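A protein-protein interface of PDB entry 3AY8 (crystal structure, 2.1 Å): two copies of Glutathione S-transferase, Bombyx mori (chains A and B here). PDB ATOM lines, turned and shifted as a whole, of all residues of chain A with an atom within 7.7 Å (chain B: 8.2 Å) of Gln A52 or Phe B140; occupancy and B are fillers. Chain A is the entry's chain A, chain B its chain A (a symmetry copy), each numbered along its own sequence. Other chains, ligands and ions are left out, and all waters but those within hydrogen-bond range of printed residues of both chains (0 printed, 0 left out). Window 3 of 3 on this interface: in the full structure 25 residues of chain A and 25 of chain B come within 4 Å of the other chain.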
ATOM      1  N   LYS A  39     -11.888 -32.484  11.226  1.00  0.00           N
ATOM      2  CA  LYS A  39     -10.773 -31.696  10.685  1.00  0.00           C
ATOM      3  C   LYS A  39     -10.876 -31.357   9.193  1.00  0.00           C
ATOM      4  O   LYS A  39     -10.384 -30.310   8.765  1.00  0.00           O
ATOM      5  CB  LYS A  39      -9.427 -32.381  10.959  1.00  0.00           C
ATOM      6  CG  LYS A  39      -9.181 -32.752  12.412  1.00  0.00           C
ATOM      7  CD  LYS A  39      -7.925 -33.606  12.550  1.00  0.00           C
ATOM      8  CE  LYS A  39      -7.940 -34.445  13.826  1.00  0.00           C
ATOM      9  NZ  LYS A  39      -8.167 -33.625  15.057  1.00  0.00           N
ATOM     10  N   PHE A  46      -9.765 -20.119  10.203  1.00  0.00           N
ATOM     11  CA  PHE A  46      -9.074 -20.668  11.374  1.00  0.00           C
ATOM     12  C   PHE A  46      -7.668 -21.186  11.055  1.00  0.00           C
ATOM     13  O   PHE A  46      -6.704 -20.823  11.733  1.00  0.00           O
ATOM     14  CB  PHE A  46      -9.912 -21.779  12.021  1.00  0.00           C
ATOM     15  CG  PHE A  46      -9.217 -22.486  13.159  1.00  0.00           C
ATOM     16  CD1 PHE A  46      -8.868 -23.828  13.049  1.00  0.00           C
ATOM     17  CD2 PHE A  46      -8.910 -21.809  14.340  1.00  0.00           C
ATOM     18  CE1 PHE A  46      -8.229 -24.490  14.098  1.00  0.00           C
ATOM     19  CE2 PHE A  46      -8.270 -22.462  15.390  1.00  0.00           C
ATOM     20  CZ  PHE A  46      -7.929 -23.804  15.265  1.00  0.00           C
ATOM     21  N   LEU A  47      -7.569 -22.032  10.025  1.00  0.00           N
ATOM     22  CA  LEU A  47      -6.304 -22.660   9.603  1.00  0.00           C
ATOM     23  C   LEU A  47      -5.224 -21.639   9.222  1.00  0.00           C
ATOM     24  O   LEU A  47      -4.028 -21.935   9.293  1.00  0.00           O
ATOM     25  CB  LEU A  47      -6.545 -23.643   8.440  1.00  0.00           C
ATOM     26  CG  LEU A  47      -7.579 -24.771   8.601  1.00  0.00           C
ATOM     27  CD1 LEU A  47      -8.012 -25.309   7.249  1.00  0.00           C
ATOM     28  CD2 LEU A  47      -7.082 -25.907   9.485  1.00  0.00           C
ATOM     29  N   LEU A  49      -4.486 -18.397  10.628  1.00  0.00           N
ATOM     30  CA  LEU A  49      -3.852 -17.466  11.572  1.00  0.00           C
ATOM     31  C   LEU A  49      -2.867 -18.023  12.610  1.00  0.00           C
ATOM     32  O   LEU A  49      -2.035 -17.272  13.119  1.00  0.00           O
ATOM     33  CB  LEU A  49      -4.908 -16.586  12.265  1.00  0.00           C
ATOM     34  CG  LEU A  49      -6.280 -17.126  12.687  1.00  0.00           C
ATOM     35  CD1 LEU A  49      -6.178 -18.202  13.757  1.00  0.00           C
ATOM     36  CD2 LEU A  49      -7.146 -15.972  13.171  1.00  0.00           C
ATOM     37  N   ASN A  50      -2.954 -19.318  12.917  1.00  0.00           N
ATOM     38  CA  ASN A  50      -2.153 -19.924  13.994  1.00  0.00           C
ATOM     39  C   ASN A  50      -1.279 -21.087  13.485  1.00  0.00           C
ATOM     40  O   ASN A  50      -1.755 -21.914  12.691  1.00  0.00           O
ATOM     41  CB  ASN A  50      -3.089 -20.402  15.125  1.00  0.00           C
ATOM     42  CG  ASN A  50      -2.406 -20.467  16.506  1.00  0.00           C
ATOM     43  OD1 ASN A  50      -1.197 -20.687  16.625  1.00  0.00           O
ATOM     44  ND2 ASN A  50      -3.209 -20.301  17.559  1.00  0.00           N
ATOM     45  N   PRO A  51       0.004 -21.141  13.920  1.00  0.00           N
ATOM     46  CA  PRO A  51       0.911 -22.270  13.678  1.00  0.00           C
ATOM     47  C   PRO A  51       0.233 -23.641  13.490  1.00  0.00           C
ATOM     48  O   PRO A  51       0.333 -24.213  12.399  1.00  0.00           O
ATOM     49  CB  PRO A  51       1.816 -22.234  14.911  1.00  0.00           C
ATOM     50  CG  PRO A  51       1.914 -20.727  15.233  1.00  0.00           C
ATOM     51  CD  PRO A  51       0.752 -20.021  14.526  1.00  0.00           C
ATOM     52  N   GLN A  52      -0.445 -24.159  14.516  1.00  0.00           N
ATOM     53  CA  GLN A  52      -1.313 -25.335  14.332  1.00  0.00           C
ATOM     54  C   GLN A  52      -2.735 -25.124  14.885  1.00  0.00           C
ATOM     55  O   GLN A  52      -3.057 -24.049  15.408  1.00  0.00           O
ATOM     56  CB  GLN A  52      -0.676 -26.592  14.926  1.00  0.00           C
ATOM     57  CG  GLN A  52      -1.240 -27.887  14.369  1.00  0.00           C
ATOM     58  CD  GLN A  52      -1.125 -29.044  15.342  1.00  0.00           C
ATOM     59  OE1 GLN A  52      -0.049 -29.314  15.884  1.00  0.00           O
ATOM     60  NE2 GLN A  52      -2.234 -29.746  15.560  1.00  0.00           N
ATOM     61  N   HIS A  53      -3.577 -26.155  14.754  1.00  0.00           N
ATOM     62  CA  HIS A  53      -4.981 -26.105  15.183  1.00  0.00           C
ATOM     63  C   HIS A  53      -5.145 -25.910  16.706  1.00  0.00           C
ATOM     64  O   HIS A  53      -5.581 -26.828  17.402  1.00  0.00           O
ATOM     65  CB  HIS A  53      -5.752 -27.379  14.746  1.00  0.00           C
ATOM     66  CG  HIS A  53      -5.289 -27.986  13.452  1.00  0.00           C
ATOM     67  ND1 HIS A  53      -5.491 -27.387  12.223  1.00  0.00           N
ATOM     68  CD2 HIS A  53      -4.664 -29.162  13.195  1.00  0.00           C
ATOM     69  CE1 HIS A  53      -4.992 -28.157  11.271  1.00  0.00           C
ATOM     70  NE2 HIS A  53      -4.484 -29.241  11.835  1.00  0.00           N
ATOM     71  N   CYS A  54      -4.806 -24.729  17.222  1.00  0.00           N
ATOM     72  CA  CYS A  54      -4.970 -24.471  18.653  1.00  0.00           C
ATOM     73  C   CYS A  54      -6.323 -23.839  18.974  1.00  0.00           C
ATOM     74  O   CYS A  54      -6.695 -22.811  18.411  1.00  0.00           O
ATOM     75  CB  CYS A  54      -3.818 -23.623  19.202  1.00  0.00           C
ATOM     76  SG  CYS A  54      -2.218 -24.479  19.210  1.00  0.00           S
ATOM     77  N   VAL A  55      -7.057 -24.493  19.878  1.00  0.00           N
ATOM     78  CA  VAL A  55      -8.325 -23.973  20.385  1.00  0.00           C
ATOM     79  C   VAL A  55      -8.283 -23.986  21.927  1.00  0.00           C
ATOM     80  O   VAL A  55      -7.849 -24.971  22.530  1.00  0.00           O
ATOM     81  CB  VAL A  55      -9.548 -24.771  19.837  1.00  0.00           C
ATOM     82  CG1 VAL A  55     -10.847 -24.258  20.428  1.00  0.00           C
ATOM     83  CG2 VAL A  55      -9.623 -24.693  18.311  1.00  0.00           C
ATOM     84  N   THR A  57      -8.503 -19.937  20.461  1.00  0.00           N
ATOM     85  CA  THR A  57      -7.629 -18.905  19.913  1.00  0.00           C
ATOM     86  C   THR A  57      -8.426 -17.602  19.889  1.00  0.00           C
ATOM     87  O   THR A  57      -9.568 -17.570  19.419  1.00  0.00           O
ATOM     88  CB  THR A  57      -7.154 -19.265  18.492  1.00  0.00           C
ATOM     89  OG1 THR A  57      -6.275 -20.392  18.545  1.00  0.00           O
ATOM     90  CG2 THR A  57      -6.430 -18.088  17.807  1.00  0.00           C
ATOM     91  N   TRP A  66      -3.308 -17.727  21.732  1.00  0.00           N
ATOM     92  CA  TRP A  66      -3.887 -18.971  22.217  1.00  0.00           C
ATOM     93  C   TRP A  66      -3.525 -19.177  23.686  1.00  0.00           C
ATOM     94  O   TRP A  66      -2.893 -18.303  24.301  1.00  0.00           O
ATOM     95  CB  TRP A  66      -3.512 -20.163  21.324  1.00  0.00           C
ATOM     96  CG  TRP A  66      -2.038 -20.333  21.089  1.00  0.00           C
ATOM     97  CD1 TRP A  66      -1.289 -19.726  20.125  1.00  0.00           C
ATOM     98  CD2 TRP A  66      -1.142 -21.180  21.821  1.00  0.00           C
ATOM     99  NE1 TRP A  66       0.027 -20.135  20.213  1.00  0.00           N
ATOM    100  CE2 TRP A  66       0.140 -21.031  21.245  1.00  0.00           C
ATOM    101  CE3 TRP A  66      -1.299 -22.064  22.903  1.00  0.00           C
ATOM    102  CZ2 TRP A  66       1.265 -21.725  21.723  1.00  0.00           C
ATOM    103  CZ3 TRP A  66      -0.165 -22.753  23.384  1.00  0.00           C
ATOM    104  CH2 TRP A  66       1.090 -22.577  22.792  1.00  0.00           C
ATOM    105  N   ARG B  99       3.488 -18.670  26.872  1.00  0.00           N
ATOM    106  CA  ARG B  99       4.601 -19.622  26.930  1.00  0.00           C
ATOM    107  C   ARG B  99       4.713 -20.285  28.312  1.00  0.00           C
ATOM    108  O   ARG B  99       5.081 -21.453  28.405  1.00  0.00           O
ATOM    109  CB  ARG B  99       5.950 -18.970  26.551  1.00  0.00           C
ATOM    110  CG  ARG B  99       5.958 -18.192  25.241  1.00  0.00           C
ATOM    111  CD  ARG B  99       5.501 -18.961  24.023  1.00  0.00           C
ATOM    112  NE  ARG B  99       6.083 -18.380  22.808  1.00  0.00           N
ATOM    113  CZ  ARG B  99       5.446 -18.202  21.653  1.00  0.00           C
ATOM    114  NH1 ARG B  99       4.181 -18.544  21.517  1.00  0.00           N
ATOM    115  NH2 ARG B  99       6.092 -17.679  20.620  1.00  0.00           N
ATOM    116  N   PHE B 102       2.095 -22.868  28.377  1.00  0.00           N
ATOM    117  CA  PHE B 102       2.659 -23.952  27.557  1.00  0.00           C
ATOM    118  C   PHE B 102       3.654 -24.805  28.361  1.00  0.00           C
ATOM    119  O   PHE B 102       3.603 -26.029  28.304  1.00  0.00           O
ATOM    120  CB  PHE B 102       3.280 -23.370  26.280  1.00  0.00           C
ATOM    121  CG  PHE B 102       4.126 -24.340  25.503  1.00  0.00           C
ATOM    122  CD1 PHE B 102       3.553 -25.171  24.536  1.00  0.00           C
ATOM    123  CD2 PHE B 102       5.498 -24.416  25.726  1.00  0.00           C
ATOM    124  CE1 PHE B 102       4.344 -26.064  23.817  1.00  0.00           C
ATOM    125  CE2 PHE B 102       6.305 -25.312  24.991  1.00  0.00           C
ATOM    126  CZ  PHE B 102       5.730 -26.122  24.040  1.00  0.00           C
ATOM    127  N   SER B 106       1.834 -28.391  28.918  1.00  0.00           N
ATOM    128  CA  SER B 106       2.285 -29.300  27.846  1.00  0.00           C
ATOM    129  C   SER B 106       3.694 -29.824  28.089  1.00  0.00           C
ATOM    130  O   SER B 106       3.913 -31.031  28.131  1.00  0.00           O
ATOM    131  CB  SER B 106       2.249 -28.599  26.469  1.00  0.00           C
ATOM    132  OG  SER B 106       0.931 -28.241  26.131  1.00  0.00           O
ATOM    133  N   LYS B 110       4.584 -33.455  30.137  1.00  0.00           N
ATOM    134  CA  LYS B 110       4.993 -34.599  29.321  1.00  0.00           C
ATOM    135  C   LYS B 110       6.372 -35.147  29.710  1.00  0.00           C
ATOM    136  O   LYS B 110       6.631 -36.335  29.565  1.00  0.00           O
ATOM    137  CB  LYS B 110       4.935 -34.227  27.842  1.00  0.00           C
ATOM    138  CG  LYS B 110       3.495 -34.106  27.327  1.00  0.00           C
ATOM    139  CD  LYS B 110       3.451 -33.614  25.887  1.00  0.00           C
ATOM    140  CE  LYS B 110       2.016 -33.156  25.519  1.00  0.00           C
ATOM    141  NZ  LYS B 110       1.933 -33.020  24.041  1.00  0.00           N
ATOM    142  N   LEU B 134       5.787 -36.103  23.930  1.00  0.00           N
ATOM    143  CA  LEU B 134       6.749 -35.065  24.252  1.00  0.00           C
ATOM    144  C   LEU B 134       7.351 -34.437  22.985  1.00  0.00           C
ATOM    145  O   LEU B 134       7.462 -33.228  22.893  1.00  0.00           O
ATOM    146  CB  LEU B 134       7.868 -35.584  25.176  1.00  0.00           C
ATOM    147  CG  LEU B 134       8.977 -34.567  25.511  1.00  0.00           C
ATOM    148  CD1 LEU B 134       8.437 -33.260  26.135  1.00  0.00           C
ATOM    149  CD2 LEU B 134      10.058 -35.187  26.407  1.00  0.00           C
ATOM    150  N   ASN B 135       7.735 -35.270  22.022  1.00  0.00           N
ATOM    151  CA  ASN B 135       8.310 -34.776  20.769  1.00  0.00           C
ATOM    152  C   ASN B 135       7.378 -33.843  19.990  1.00  0.00           C
ATOM    153  O   ASN B 135       7.831 -32.873  19.394  1.00  0.00           O
ATOM    154  CB  ASN B 135       8.826 -35.947  19.912  1.00  0.00           C
ATOM    155  CG  ASN B 135      10.227 -36.407  20.328  1.00  0.00           C
ATOM    156  OD1 ASN B 135      10.619 -37.562  20.107  1.00  0.00           O
ATOM    157  ND2 ASN B 135      10.987 -35.508  20.924  1.00  0.00           N
ATOM    158  N   SER B 136       6.067 -34.097  20.047  1.00  0.00           N
ATOM    159  CA  SER B 136       5.094 -33.189  19.451  1.00  0.00           C
ATOM    160  C   SER B 136       5.102 -31.798  20.127  1.00  0.00           C
ATOM    161  O   SER B 136       4.973 -30.750  19.457  1.00  0.00           O
ATOM    162  CB  SER B 136       3.694 -33.815  19.517  1.00  0.00           C
ATOM    163  OG  SER B 136       2.706 -32.833  19.256  1.00  0.00           O
ATOM    164  N   THR B 137       5.260 -31.795  21.450  1.00  0.00           N
ATOM    165  CA  THR B 137       5.373 -30.545  22.207  1.00  0.00           C
ATOM    166  C   THR B 137       6.709 -29.864  21.934  1.00  0.00           C
ATOM    167  O   THR B 137       6.763 -28.643  21.769  1.00  0.00           O
ATOM    168  CB  THR B 137       5.117 -30.782  23.711  1.00  0.00           C
ATOM    169  OG1 THR B 137       3.717 -31.026  23.877  1.00  0.00           O
ATOM    170  CG2 THR B 137       5.510 -29.544  24.554  1.00  0.00           C
ATOM    171  N   LEU B 138       7.781 -30.657  21.822  1.00  0.00           N
ATOM    172  CA  LEU B 138       9.076 -30.073  21.426  1.00  0.00           C
ATOM    173  C   LEU B 138       9.029 -29.404  20.056  1.00  0.00           C
ATOM    174  O   LEU B 138       9.677 -28.380  19.828  1.00  0.00           O
ATOM    175  CB  LEU B 138      10.200 -31.120  21.471  1.00  0.00           C
ATOM    176  CG  LEU B 138      10.510 -31.720  22.855  1.00  0.00           C
ATOM    177  CD1 LEU B 138      11.751 -32.607  22.789  1.00  0.00           C
ATOM    178  CD2 LEU B 138      10.663 -30.615  23.919  1.00  0.00           C
ATOM    179  N   SER B 139       8.276 -29.999  19.133  1.00  0.00           N
ATOM    180  CA  SER B 139       8.162 -29.451  17.787  1.00  0.00           C
ATOM    181  C   SER B 139       7.539 -28.055  17.793  1.00  0.00           C
ATOM    182  O   SER B 139       7.973 -27.176  17.062  1.00  0.00           O
ATOM    183  CB  SER B 139       7.364 -30.403  16.885  1.00  0.00           C
ATOM    184  OG  SER B 139       7.257 -29.844  15.590  1.00  0.00           O
ATOM    185  N   PHE B 140       6.526 -27.874  18.637  1.00  0.00           N
ATOM    186  CA  PHE B 140       5.877 -26.586  18.853  1.00  0.00           C
ATOM    187  C   PHE B 140       6.864 -25.573  19.424  1.00  0.00           C
ATOM    188  O   PHE B 140       6.931 -24.442  18.952  1.00  0.00           O
ATOM    189  CB  PHE B 140       4.705 -26.751  19.812  1.00  0.00           C
ATOM    190  CG  PHE B 140       3.367 -26.671  19.162  1.00  0.00           C
ATOM    191  CD1 PHE B 140       2.586 -25.529  19.305  1.00  0.00           C
ATOM    192  CD2 PHE B 140       2.873 -27.738  18.415  1.00  0.00           C
ATOM    193  CE1 PHE B 140       1.328 -25.445  18.707  1.00  0.00           C
ATOM    194  CE2 PHE B 140       1.617 -27.667  17.808  1.00  0.00           C
ATOM    195  CZ  PHE B 140       0.841 -26.524  17.960  1.00  0.00           C
ATOM    196  N   LEU B 141       7.628 -25.989  20.434  1.00  0.00           N
ATOM    197  CA  LEU B 141       8.662 -25.131  21.018  1.00  0.00           C
ATOM    198  C   LEU B 141       9.678 -24.742  19.942  1.00  0.00           C
ATOM    199  O   LEU B 141      10.100 -23.602  19.867  1.00  0.00           O
ATOM    200  CB  LEU B 141       9.378 -25.831  22.182  1.00  0.00           C
ATOM    201  CG  LEU B 141      10.548 -25.064  22.830  1.00  0.00           C
ATOM    202  CD1 LEU B 141      10.152 -23.607  23.276  1.00  0.00           C
ATOM    203  CD2 LEU B 141      11.160 -25.858  24.000  1.00  0.00           C
ATOM    204  N   ASN B 142      10.072 -25.712  19.129  1.00  0.00           N
ATOM    205  CA  ASN B 142      11.018 -25.464  18.053  1.00  0.00           C
ATOM    206  C   ASN B 142      10.513 -24.374  17.092  1.00  0.00           C
ATOM    207  O   ASN B 142      11.299 -23.560  16.616  1.00  0.00           O
ATOM    208  CB  ASN B 142      11.340 -26.753  17.301  1.00  0.00           C
ATOM    209  CG  ASN B 142      12.412 -26.545  16.233  1.00  0.00           C
ATOM    210  OD1 ASN B 142      13.558 -26.218  16.533  1.00  0.00           O
ATOM    211  ND2 ASN B 142      12.034 -26.732  14.986  1.00  0.00           N
ATOM    212  N   GLN B 143       9.203 -24.359  16.845  1.00  0.00           N
ATOM    213  CA  GLN B 143       8.549 -23.310  16.040  1.00  0.00           C
ATOM    214  C   GLN B 143       8.517 -21.937  16.719  1.00  0.00           C
ATOM    215  O   GLN B 143       8.803 -20.925  16.060  1.00  0.00           O
ATOM    216  CB  GLN B 143       7.135 -23.721  15.593  1.00  0.00           C
ATOM    217  CG  GLN B 143       7.119 -24.826  14.529  1.00  0.00           C
ATOM    218  CD  GLN B 143       8.063 -24.533  13.357  1.00  0.00           C
ATOM    219  OE1 GLN B 143       7.955 -23.502  12.694  1.00  0.00           O
ATOM    220  NE2 GLN B 143       8.995 -25.437  13.114  1.00  0.00           N
ATOM    221  N   PHE B 144       8.191 -21.889  18.017  1.00  0.00           N
ATOM    222  CA  PHE B 144       8.278 -20.616  18.770  1.00  0.00           C
ATOM    223  C   PHE B 144       9.629 -19.953  18.504  1.00  0.00           C
ATOM    224  O   PHE B 144       9.710 -18.749  18.260  1.00  0.00           O
ATOM    225  CB  PHE B 144       8.150 -20.816  20.297  1.00  0.00           C
ATOM    226  CG  PHE B 144       6.865 -21.462  20.746  1.00  0.00           C
ATOM    227  CD1 PHE B 144       5.706 -21.404  19.971  1.00  0.00           C
ATOM    228  CD2 PHE B 144       6.808 -22.092  21.978  1.00  0.00           C
ATOM    229  CE1 PHE B 144       4.520 -22.017  20.411  1.00  0.00           C
ATOM    230  CE2 PHE B 144       5.639 -22.686  22.428  1.00  0.00           C
ATOM    231  CZ  PHE B 144       4.500 -22.660  21.644  1.00  0.00           C
ATOM    232  N   LEU B 145      10.680 -20.765  18.541  1.00  0.00           N
ATOM    233  CA  LEU B 145      12.056 -20.287  18.434  1.00  0.00           C
ATOM    234  C   LEU B 145      12.537 -20.079  16.986  1.00  0.00           C
ATOM    235  O   LEU B 145      13.702 -19.764  16.756  1.00  0.00           O
ATOM    236  CB  LEU B 145      12.986 -21.244  19.183  1.00  0.00           C
ATOM    237  CG  LEU B 145      12.802 -21.267  20.701  1.00  0.00           C
ATOM    238  CD1 LEU B 145      13.423 -22.520  21.289  1.00  0.00           C
ATOM    239  CD2 LEU B 145      13.381 -19.996  21.352  1.00  0.00           C
ATOM    240  N   GLU B 146      11.640 -20.268  16.023  1.00  0.00           N
ATOM    241  CA  GLU B 146      11.924 -19.967  14.619  1.00  0.00           C
ATOM    242  C   GLU B 146      11.696 -18.477  14.376  1.00  0.00           C
ATOM    243  O   GLU B 146      12.409 -17.849  13.593  1.00  0.00           O
ATOM    244  CB  GLU B 146      11.012 -20.795  13.696  1.00  0.00           C
ATOM    245  CG  GLU B 146      11.176 -20.504  12.186  1.00  0.00           C
ATOM    246  CD  GLU B 146      12.500 -20.988  11.636  1.00  0.00           C
ATOM    247  OE1 GLU B 146      13.033 -22.003  12.140  1.00  0.00           O
ATOM    248  OE2 GLU B 146      13.018 -20.350  10.699  1.00  0.00           O
ATOM    249  N   LYS B 147      10.701 -17.929  15.067  1.00  0.00           N
ATOM    250  CA  LYS B 147      10.283 -16.541  14.902  1.00  0.00           C
ATOM    251  C   LYS B 147      11.204 -15.575  15.646  1.00  0.00           C
ATOM    252  O   LYS B 147      11.635 -14.566  15.083  1.00  0.00           O
ATOM    253  CB  LYS B 147       8.839 -16.371  15.388  1.00  0.00           C
ATOM    254  CG  LYS B 147       7.865 -17.382  14.798  1.00  0.00           C
ATOM    255  CD  LYS B 147       6.449 -17.200  15.351  1.00  0.00           C
ATOM    256  CE  LYS B 147       5.443 -18.065  14.604  1.00  0.00           C
ATOM    257  NZ  LYS B 147       5.647 -19.525  14.844  1.00  0.00           N
ATOM    258  N   VAL B 151      12.164 -17.529  23.663  1.00  0.00           N
ATOM    259  CA  VAL B 151      10.846 -18.185  23.494  1.00  0.00           C
ATOM    260  C   VAL B 151       9.680 -17.222  23.252  1.00  0.00           C
ATOM    261  O   VAL B 151       8.717 -17.575  22.572  1.00  0.00           O
ATOM    262  CB  VAL B 151      10.444 -19.162  24.661  1.00  0.00           C
ATOM    263  CG1 VAL B 151      11.400 -20.337  24.789  1.00  0.00           C
ATOM    264  CG2 VAL B 151      10.278 -18.426  25.975  1.00  0.00           C
ATOM    265  N   PHE B 180      15.283 -30.639  16.119  1.00  0.00           N
ATOM    266  CA  PHE B 180      14.871 -29.293  16.516  1.00  0.00           C
ATOM    267  C   PHE B 180      16.032 -28.313  16.629  1.00  0.00           C
ATOM    268  O   PHE B 180      16.460 -27.979  17.742  1.00  0.00           O
ATOM    269  CB  PHE B 180      14.047 -29.341  17.812  1.00  0.00           C
ATOM    270  CG  PHE B 180      13.025 -30.444  17.842  1.00  0.00           C
ATOM    271  CD1 PHE B 180      11.970 -30.466  16.928  1.00  0.00           C
ATOM    272  CD2 PHE B 180      13.112 -31.460  18.793  1.00  0.00           C
ATOM    273  CE1 PHE B 180      11.024 -31.490  16.958  1.00  0.00           C
ATOM    274  CE2 PHE B 180      12.173 -32.484  18.835  1.00  0.00           C
ATOM    275  CZ  PHE B 180      11.125 -32.503  17.912  1.00  0.00           C
ATOM    276  N   ASN B 182      16.283 -25.139  16.310  1.00  0.00           N
ATOM    277  CA  ASN B 182      16.001 -23.887  17.050  1.00  0.00           C
ATOM    278  C   ASN B 182      16.121 -24.032  18.569  1.00  0.00           C
ATOM    279  O   ASN B 182      16.608 -23.124  19.237  1.00  0.00           O
ATOM    280  CB  ASN B 182      14.647 -23.281  16.651  1.00  0.00           C
ATOM    281  CG  ASN B 182      14.574 -22.944  15.157  1.00  0.00           C
ATOM    282  OD1 ASN B 182      15.560 -22.516  14.554  1.00  0.00           O
ATOM    283  ND2 ASN B 182      13.407 -23.136  14.567  1.00  0.00           N
ATOM    284  N   ILE B 183      15.678 -25.174  19.098  1.00  0.00           N
ATOM    285  CA  ILE B 183      15.908 -25.527  20.507  1.00  0.00           C
ATOM    286  C   ILE B 183      17.409 -25.684  20.785  1.00  0.00           C
ATOM    287  O   ILE B 183      17.909 -25.220  21.814  1.00  0.00           O
ATOM    288  CB  ILE B 183      15.153 -26.828  20.949  1.00  0.00           C
ATOM    289  CG1 ILE B 183      13.636 -26.703  20.689  1.00  0.00           C
ATOM    290  CG2 ILE B 183      15.416 -27.122  22.452  1.00  0.00           C
ATOM    291  CD1 ILE B 183      12.817 -27.942  21.057  1.00  0.00           C
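Of the 22 printed residues of chain B, 4 touch a printed residue of chain A.
Hydrophobic or aromatic side chains of chain B that line the printed part of chain A: Phe B102, Phe B140 and Phe B144.
Of the 12 printed residues of chain A, 4 touch a printed residue of chain B.
Hydrophobic or aromatic side chains of chain A within 4 Å of the printed part of chain B: Pro A51 and Trp A66.
Among the printed residues, 5 pairs touch across the chains.
Among the printed residues, no Asp or Glu carboxylate lies within 4 Å of a Lys or Arg side-chain nitrogen of the other chain.
Printed residues of chain B within 4 Å of Gln A52: Phe B140.
Of the printed residues of chain A, Phe B140 touches Gln A52 (3.0 Å) and Cys A54 (3.7 Å).
Of the printed residues of chain A, Lys B147 touches Pro A51 (3.9 Å).
Printed residues of chain B within 4 Å of Cys A54: Phe B140 (3.7 Å).
Printed residues of chain A within 4 Å of Phe B102: Trp A66.
Printed residues of chain A within 4 Å of Phe B144: Trp A66 (3.4 Å).
Ser B139 touches none of the printed residues of chain A.
Asn A50 touches none of the printed residues of chain B.
The nearest printed residue of chain A that does not touch Phe B140 is Trp A66 (4.7 Å).
O of Cys A54 lies within hydrogen-bond range of OG1 of Thr A57.
Among the printed residues, merely in contact across the chains: Pro A51 with Lys B147 (3.9 Å), Gln A52 with Phe B140 (3.0 Å), Cys A54 with Phe B140 (3.7 Å), Trp A66 with Phe B102 (3.98 Å) and Trp A66 with Phe B144 (3.4 Å).
No position is printed for both chains.
Of the 5 pairs that touch across the chains among the printed residues, none has its exchanged pair printed and touching as well.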
